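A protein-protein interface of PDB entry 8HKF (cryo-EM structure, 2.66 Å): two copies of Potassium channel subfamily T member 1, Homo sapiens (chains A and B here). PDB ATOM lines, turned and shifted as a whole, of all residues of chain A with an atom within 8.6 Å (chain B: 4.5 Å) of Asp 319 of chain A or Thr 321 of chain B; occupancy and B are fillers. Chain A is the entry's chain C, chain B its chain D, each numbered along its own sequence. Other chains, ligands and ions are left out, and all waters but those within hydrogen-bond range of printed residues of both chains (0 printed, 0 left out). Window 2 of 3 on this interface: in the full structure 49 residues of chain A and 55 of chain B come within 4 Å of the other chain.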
ATOM      1  N   LEU A 299     -38.107 -10.733 -13.743  1.00  0.00           N
ATOM      2  CA  LEU A 299     -37.177 -10.143 -14.697  1.00  0.00           C
ATOM      3  C   LEU A 299     -37.924  -9.431 -15.819  1.00  0.00           C
ATOM      4  O   LEU A 299     -38.929  -9.933 -16.330  1.00  0.00           O
ATOM      5  CB  LEU A 299     -36.266 -11.222 -15.279  1.00  0.00           C
ATOM      6  CG  LEU A 299     -34.846 -11.255 -14.720  1.00  0.00           C
ATOM      7  CD1 LEU A 299     -34.061 -12.418 -15.300  1.00  0.00           C
ATOM      8  CD2 LEU A 299     -34.161  -9.950 -14.994  1.00  0.00           C
ATOM      9  N   THR A 303     -33.804  -6.773 -19.483  1.00  0.00           N
ATOM     10  CA  THR A 303     -32.753  -7.368 -18.666  1.00  0.00           C
ATOM     11  C   THR A 303     -32.516  -8.829 -19.032  1.00  0.00           C
ATOM     12  O   THR A 303     -31.366  -9.281 -19.072  1.00  0.00           O
ATOM     13  CB  THR A 303     -33.105  -7.241 -17.185  1.00  0.00           C
ATOM     14  OG1 THR A 303     -33.316  -5.863 -16.860  1.00  0.00           O
ATOM     15  CG2 THR A 303     -31.962  -7.768 -16.337  1.00  0.00           C
ATOM     16  N   TYR A 306     -30.412  -9.046 -22.083  1.00  0.00           N
ATOM     17  CA  TYR A 306     -29.009  -8.880 -21.721  1.00  0.00           C
ATOM     18  C   TYR A 306     -28.467 -10.133 -21.048  1.00  0.00           C
ATOM     19  O   TYR A 306     -27.307 -10.508 -21.258  1.00  0.00           O
ATOM     20  CB  TYR A 306     -28.853  -7.658 -20.816  1.00  0.00           C
ATOM     21  CG  TYR A 306     -27.643  -7.692 -19.912  1.00  0.00           C
ATOM     22  CD1 TYR A 306     -26.391  -7.326 -20.384  1.00  0.00           C
ATOM     23  CD2 TYR A 306     -27.757  -8.070 -18.580  1.00  0.00           C
ATOM     24  CE1 TYR A 306     -25.284  -7.348 -19.560  1.00  0.00           C
ATOM     25  CE2 TYR A 306     -26.655  -8.095 -17.749  1.00  0.00           C
ATOM     26  CZ  TYR A 306     -25.421  -7.732 -18.244  1.00  0.00           C
ATOM     27  OH  TYR A 306     -24.319  -7.754 -17.421  1.00  0.00           O
ATOM     28  N   PHE A 307     -29.292 -10.795 -20.232  1.00  0.00           N
ATOM     29  CA  PHE A 307     -28.852 -12.005 -19.545  1.00  0.00           C
ATOM     30  C   PHE A 307     -28.508 -13.110 -20.535  1.00  0.00           C
ATOM     31  O   PHE A 307     -27.500 -13.808 -20.380  1.00  0.00           O
ATOM     32  CB  PHE A 307     -29.931 -12.480 -18.573  1.00  0.00           C
ATOM     33  CG  PHE A 307     -29.769 -13.910 -18.142  1.00  0.00           C
ATOM     34  CD1 PHE A 307     -28.794 -14.262 -17.226  1.00  0.00           C
ATOM     35  CD2 PHE A 307     -30.588 -14.902 -18.655  1.00  0.00           C
ATOM     36  CE1 PHE A 307     -28.639 -15.574 -16.827  1.00  0.00           C
ATOM     37  CE2 PHE A 307     -30.436 -16.217 -18.259  1.00  0.00           C
ATOM     38  CZ  PHE A 307     -29.461 -16.552 -17.344  1.00  0.00           C
ATOM     39  N   VAL A 310     -25.179 -12.382 -22.758  1.00  0.00           N
ATOM     40  CA  VAL A 310     -23.960 -12.708 -22.018  1.00  0.00           C
ATOM     41  C   VAL A 310     -23.900 -14.171 -21.616  1.00  0.00           C
ATOM     42  O   VAL A 310     -22.852 -14.630 -21.143  1.00  0.00           O
ATOM     43  CB  VAL A 310     -23.816 -11.829 -20.762  1.00  0.00           C
ATOM     44  CG1 VAL A 310     -23.974 -10.360 -21.120  1.00  0.00           C
ATOM     45  CG2 VAL A 310     -24.825 -12.237 -19.703  1.00  0.00           C
ATOM     46  N   THR A 311     -24.992 -14.918 -21.788  1.00  0.00           N
ATOM     47  CA  THR A 311     -24.967 -16.354 -21.529  1.00  0.00           C
ATOM     48  C   THR A 311     -24.457 -17.124 -22.741  1.00  0.00           C
ATOM     49  O   THR A 311     -23.501 -17.899 -22.635  1.00  0.00           O
ATOM     50  CB  THR A 311     -26.363 -16.846 -21.142  1.00  0.00           C
ATOM     51  OG1 THR A 311     -26.691 -16.378 -19.828  1.00  0.00           O
ATOM     52  CG2 THR A 311     -26.416 -18.367 -21.168  1.00  0.00           C
ATOM     53  N   VAL A 315     -19.954 -15.250 -21.467  1.00  0.00           N
ATOM     54  CA  VAL A 315     -19.405 -14.251 -20.557  1.00  0.00           C
ATOM     55  C   VAL A 315     -19.813 -14.561 -19.122  1.00  0.00           C
ATOM     56  O   VAL A 315     -18.971 -14.588 -18.217  1.00  0.00           O
ATOM     57  CB  VAL A 315     -19.847 -12.841 -20.985  1.00  0.00           C
ATOM     58  CG1 VAL A 315     -19.393 -11.813 -19.964  1.00  0.00           C
ATOM     59  CG2 VAL A 315     -19.290 -12.509 -22.360  1.00  0.00           C
ATOM     60  N   GLY A 316     -21.100 -14.819 -18.894  1.00  0.00           N
ATOM     61  CA  GLY A 316     -21.599 -15.175 -17.579  1.00  0.00           C
ATOM     62  C   GLY A 316     -21.344 -14.207 -16.442  1.00  0.00           C
ATOM     63  O   GLY A 316     -20.828 -14.599 -15.391  1.00  0.00           O
ATOM     64  N   TYR A 317     -21.698 -12.936 -16.643  1.00  0.00           N
ATOM     65  CA  TYR A 317     -21.443 -11.927 -15.620  1.00  0.00           C
ATOM     66  C   TYR A 317     -21.942 -12.297 -14.229  1.00  0.00           C
ATOM     67  O   TYR A 317     -21.235 -12.095 -13.234  1.00  0.00           O
ATOM     68  CB  TYR A 317     -22.026 -10.587 -16.060  1.00  0.00           C
ATOM     69  CG  TYR A 317     -21.081  -9.778 -16.911  1.00  0.00           C
ATOM     70  CD1 TYR A 317     -19.796  -9.493 -16.473  1.00  0.00           C
ATOM     71  CD2 TYR A 317     -21.471  -9.307 -18.157  1.00  0.00           C
ATOM     72  CE1 TYR A 317     -18.927  -8.758 -17.248  1.00  0.00           C
ATOM     73  CE2 TYR A 317     -20.608  -8.570 -18.938  1.00  0.00           C
ATOM     74  CZ  TYR A 317     -19.339  -8.299 -18.479  1.00  0.00           C
ATOM     75  OH  TYR A 317     -18.480  -7.566 -19.257  1.00  0.00           O
ATOM     76  N   GLY A 318     -23.153 -12.837 -14.138  1.00  0.00           N
ATOM     77  CA  GLY A 318     -23.706 -13.248 -12.867  1.00  0.00           C
ATOM     78  C   GLY A 318     -24.462 -12.181 -12.110  1.00  0.00           C
ATOM     79  O   GLY A 318     -25.003 -12.476 -11.036  1.00  0.00           O
ATOM     80  N   ASP A 319     -24.513 -10.947 -12.621  1.00  0.00           N
ATOM     81  CA  ASP A 319     -25.317  -9.918 -11.969  1.00  0.00           C
ATOM     82  C   ASP A 319     -26.800 -10.261 -12.016  1.00  0.00           C
ATOM     83  O   ASP A 319     -27.544  -9.919 -11.091  1.00  0.00           O
ATOM     84  CB  ASP A 319     -25.058  -8.554 -12.612  1.00  0.00           C
ATOM     85  CG  ASP A 319     -25.359  -8.540 -14.099  1.00  0.00           C
ATOM     86  OD1 ASP A 319     -25.621  -9.620 -14.669  1.00  0.00           O
ATOM     87  OD2 ASP A 319     -25.335  -7.445 -14.697  1.00  0.00           O
ATOM     88  N   VAL A 320     -27.243 -10.925 -13.080  1.00  0.00           N
ATOM     89  CA  VAL A 320     -28.597 -11.452 -13.187  1.00  0.00           C
ATOM     90  C   VAL A 320     -28.482 -12.954 -13.413  1.00  0.00           C
ATOM     91  O   VAL A 320     -27.899 -13.397 -14.410  1.00  0.00           O
ATOM     92  CB  VAL A 320     -29.404 -10.774 -14.306  1.00  0.00           C
ATOM     93  CG1 VAL A 320     -28.611 -10.729 -15.607  1.00  0.00           C
ATOM     94  CG2 VAL A 320     -30.722 -11.491 -14.511  1.00  0.00           C
ATOM     95  N   THR A 321     -29.016 -13.737 -12.483  1.00  0.00           N
ATOM     96  CA  THR A 321     -28.927 -15.185 -12.530  1.00  0.00           C
ATOM     97  C   THR A 321     -30.279 -15.795 -12.197  1.00  0.00           C
ATOM     98  O   THR A 321     -31.060 -15.204 -11.444  1.00  0.00           O
ATOM     99  CB  THR A 321     -27.865 -15.702 -11.545  1.00  0.00           C
ATOM    100  OG1 THR A 321     -27.986 -17.123 -11.395  1.00  0.00           O
ATOM    101  CG2 THR A 321     -28.026 -15.035 -10.187  1.00  0.00           C
ATOM    102  N   PRO A 322     -30.593 -16.962 -12.758  1.00  0.00           N
ATOM    103  CA  PRO A 322     -31.836 -17.645 -12.381  1.00  0.00           C
ATOM    104  C   PRO A 322     -31.811 -18.047 -10.913  1.00  0.00           C
ATOM    105  O   PRO A 322     -30.902 -18.746 -10.459  1.00  0.00           O
ATOM    106  CB  PRO A 322     -31.865 -18.868 -13.306  1.00  0.00           C
ATOM    107  CG  PRO A 322     -30.443 -19.057 -13.736  1.00  0.00           C
ATOM    108  CD  PRO A 322     -29.878 -17.676 -13.829  1.00  0.00           C
ATOM    109  N   LYS A 323     -32.820 -17.596 -10.171  1.00  0.00           N
ATOM    110  CA  LYS A 323     -32.864 -17.798  -8.730  1.00  0.00           C
ATOM    111  C   LYS A 323     -33.799 -18.917  -8.299  1.00  0.00           C
ATOM    112  O   LYS A 323     -33.924 -19.174  -7.101  1.00  0.00           O
ATOM    113  CB  LYS A 323     -33.264 -16.496  -8.028  1.00  0.00           C
ATOM    114  CG  LYS A 323     -32.971 -15.241  -8.834  1.00  0.00           C
ATOM    115  CD  LYS A 323     -33.127 -13.986  -7.988  1.00  0.00           C
ATOM    116  CE  LYS A 323     -32.438 -14.137  -6.641  1.00  0.00           C
ATOM    117  NZ  LYS A 323     -32.221 -12.821  -5.980  1.00  0.00           N
ATOM    118  N   PHE B 307     -12.652  -3.992 -17.288  1.00  0.00           N
ATOM    119  CA  PHE B 307     -13.977  -4.559 -17.507  1.00  0.00           C
ATOM    120  C   PHE B 307     -14.101  -5.152 -18.905  1.00  0.00           C
ATOM    121  O   PHE B 307     -14.618  -6.261 -19.079  1.00  0.00           O
ATOM    122  CB  PHE B 307     -15.042  -3.483 -17.285  1.00  0.00           C
ATOM    123  CG  PHE B 307     -16.401  -3.855 -17.801  1.00  0.00           C
ATOM    124  CD1 PHE B 307     -17.233  -4.678 -17.066  1.00  0.00           C
ATOM    125  CD2 PHE B 307     -16.848  -3.380 -19.023  1.00  0.00           C
ATOM    126  CE1 PHE B 307     -18.485  -5.021 -17.535  1.00  0.00           C
ATOM    127  CE2 PHE B 307     -18.097  -3.723 -19.499  1.00  0.00           C
ATOM    128  CZ  PHE B 307     -18.917  -4.543 -18.754  1.00  0.00           C
ATOM    129  N   GLY B 318     -17.662 -10.367 -13.220  1.00  0.00           N
ATOM    130  CA  GLY B 318     -18.861  -9.846 -12.598  1.00  0.00           C
ATOM    131  C   GLY B 318     -18.639  -8.885 -11.449  1.00  0.00           C
ATOM    132  O   GLY B 318     -19.621  -8.362 -10.908  1.00  0.00           O
ATOM    133  N   ASP B 319     -17.388  -8.643 -11.048  1.00  0.00           N
ATOM    134  CA  ASP B 319     -17.131  -7.662 -10.000  1.00  0.00           C
ATOM    135  C   ASP B 319     -17.513  -6.258 -10.447  1.00  0.00           C
ATOM    136  O   ASP B 319     -17.973  -5.449  -9.633  1.00  0.00           O
ATOM    137  CB  ASP B 319     -15.661  -7.717  -9.579  1.00  0.00           C
ATOM    138  CG  ASP B 319     -14.714  -7.460 -10.734  1.00  0.00           C
ATOM    139  OD1 ASP B 319     -15.185  -7.392 -11.889  1.00  0.00           O
ATOM    140  OD2 ASP B 319     -13.499  -7.328 -10.488  1.00  0.00           O
ATOM    141  N   VAL B 320     -17.323  -5.950 -11.727  1.00  0.00           N
ATOM    142  CA  VAL B 320     -17.766  -4.697 -12.326  1.00  0.00           C
ATOM    143  C   VAL B 320     -18.737  -5.060 -13.440  1.00  0.00           C
ATOM    144  O   VAL B 320     -18.360  -5.745 -14.398  1.00  0.00           O
ATOM    145  CB  VAL B 320     -16.597  -3.863 -12.871  1.00  0.00           C
ATOM    146  CG1 VAL B 320     -17.119  -2.669 -13.649  1.00  0.00           C
ATOM    147  CG2 VAL B 320     -15.695  -3.412 -11.734  1.00  0.00           C
ATOM    148  N   THR B 321     -19.980  -4.610 -13.319  1.00  0.00           N
ATOM    149  CA  THR B 321     -21.007  -4.921 -14.297  1.00  0.00           C
ATOM    150  C   THR B 321     -21.800  -3.669 -14.635  1.00  0.00           C
ATOM    151  O   THR B 321     -21.921  -2.762 -13.805  1.00  0.00           O
ATOM    152  CB  THR B 321     -21.960  -6.007 -13.774  1.00  0.00           C
ATOM    153  OG1 THR B 321     -22.164  -5.830 -12.367  1.00  0.00           O
ATOM    154  CG2 THR B 321     -21.382  -7.389 -14.028  1.00  0.00           C
ATOM    155  N   PRO B 322     -22.339  -3.586 -15.850  1.00  0.00           N
ATOM    156  CA  PRO B 322     -23.213  -2.454 -16.187  1.00  0.00           C
ATOM    157  C   PRO B 322     -24.487  -2.491 -15.357  1.00  0.00           C
ATOM    158  O   PRO B 322     -25.215  -3.485 -15.347  1.00  0.00           O
ATOM    159  CB  PRO B 322     -23.498  -2.660 -17.679  1.00  0.00           C
ATOM    160  CG  PRO B 322     -23.250  -4.113 -17.918  1.00  0.00           C
ATOM    161  CD  PRO B 322     -22.129  -4.482 -16.999  1.00  0.00           C
ATOM    162  N   LYS B 323     -24.750  -1.392 -14.653  1.00  0.00           N
ATOM    163  CA  LYS B 323     -25.873  -1.313 -13.729  1.00  0.00           C
ATOM    164  C   LYS B 323     -27.063  -0.545 -14.289  1.00  0.00           C
ATOM    165  O   LYS B 323     -28.062  -0.381 -13.583  1.00  0.00           O
ATOM    166  CB  LYS B 323     -25.424  -0.675 -12.412  1.00  0.00           C
ATOM    167  CG  LYS B 323     -24.076  -1.171 -11.913  1.00  0.00           C
ATOM    168  CD  LYS B 323     -24.242  -2.304 -10.915  1.00  0.00           C
ATOM    169  CE  LYS B 323     -24.835  -1.809  -9.607  1.00  0.00           C
ATOM    170  NZ  LYS B 323     -23.825  -1.115  -8.761  1.00  0.00           N
ATOM    171  N   GLN B 328     -25.916  -1.840 -20.400  1.00  0.00           N
ATOM    172  CA  GLN B 328     -26.185  -3.246 -20.683  1.00  0.00           C
ATOM    173  C   GLN B 328     -26.416  -3.466 -22.171  1.00  0.00           C
ATOM    174  O   GLN B 328     -25.931  -4.443 -22.753  1.00  0.00           O
ATOM    175  CB  GLN B 328     -27.392  -3.724 -19.875  1.00  0.00           C
ATOM    176  CG  GLN B 328     -27.204  -3.656 -18.372  1.00  0.00           C
ATOM    177  CD  GLN B 328     -28.425  -4.128 -17.612  1.00  0.00           C
ATOM    178  OE1 GLN B 328     -29.549  -4.042 -18.106  1.00  0.00           O
ATOM    179  NE2 GLN B 328     -28.212  -4.632 -16.402  1.00  0.00           N
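Of the printed residues of chain B, Asp 319 of chain A touches Thr 321 (3.8 Å). Of the printed residues of chain A, Thr 321 of chain B touches Tyr 317 and Asp 319. Of the printed residues of chain A, Pro 322 of chain B touches Tyr 306 (3.8 Å). Printed residues of chain A within 4 Å of Gln 328 of chain B: Tyr 306 (3.8 Å). The nearest printed residue of chain B that does not touch Asp 319 of chain A is Pro 322 of chain B (4.01 Å). The nearest printed residue of chain A that does not touch Gln 328 of chain B is Thr 303 of chain A (4.4 Å).
Among the printed residues, pairs that only touch across the chains: Tyr 306 of chain A with Pro 322 of chain B (3.8 Å), Tyr 306 of chain A with Gln 328 of chain B (3.8 Å), Tyr 317 of chain A with Phe 307 of chain B (3.1 Å), Tyr 317 of chain A with Gly 318 of chain B (3.3 Å), Tyr 317 of chain A with Thr 321 of chain B (3.6 Å) and Asp 319 of chain A with Thr 321 of chain B (3.8 Å).
Asp 319 of chain A touches Thr 321 of chain B, but with the chains exchanged Thr 321 of chain A does not touch Asp 319 of chain B (12.4 Å). Positions printed for both chains: 307, 318, 319, 320, 321, 322 and 323. Of the 6 pairs that touch across the chains among the printed residues, none has its exchanged pair printed and touching as well.
OD2 of Asp 319 of chain A lies within hydrogen-bond range of OH of Tyr 306 of chain A, at 2.9 Å. The side-chain amide nitrogen (NE2) of Gln 328 of chain B sits at hydrogen-bond distance from the backbone carbonyl oxygen (O) of Pro 322 of chain B (3.4 Å).
Of the 8 printed residues of chain B, 5 touch a printed residue of chain A. Hydrophobic or aromatic side chains of chain B that line the printed part of chain A: Phe 307 and Pro 322. Of the 15 printed residues of chain A, 3 touch a printed residue of chain B. Printed residues of chain A that touch a printed residue of chain B: Tyr 306, Tyr 317 and Asp 319.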
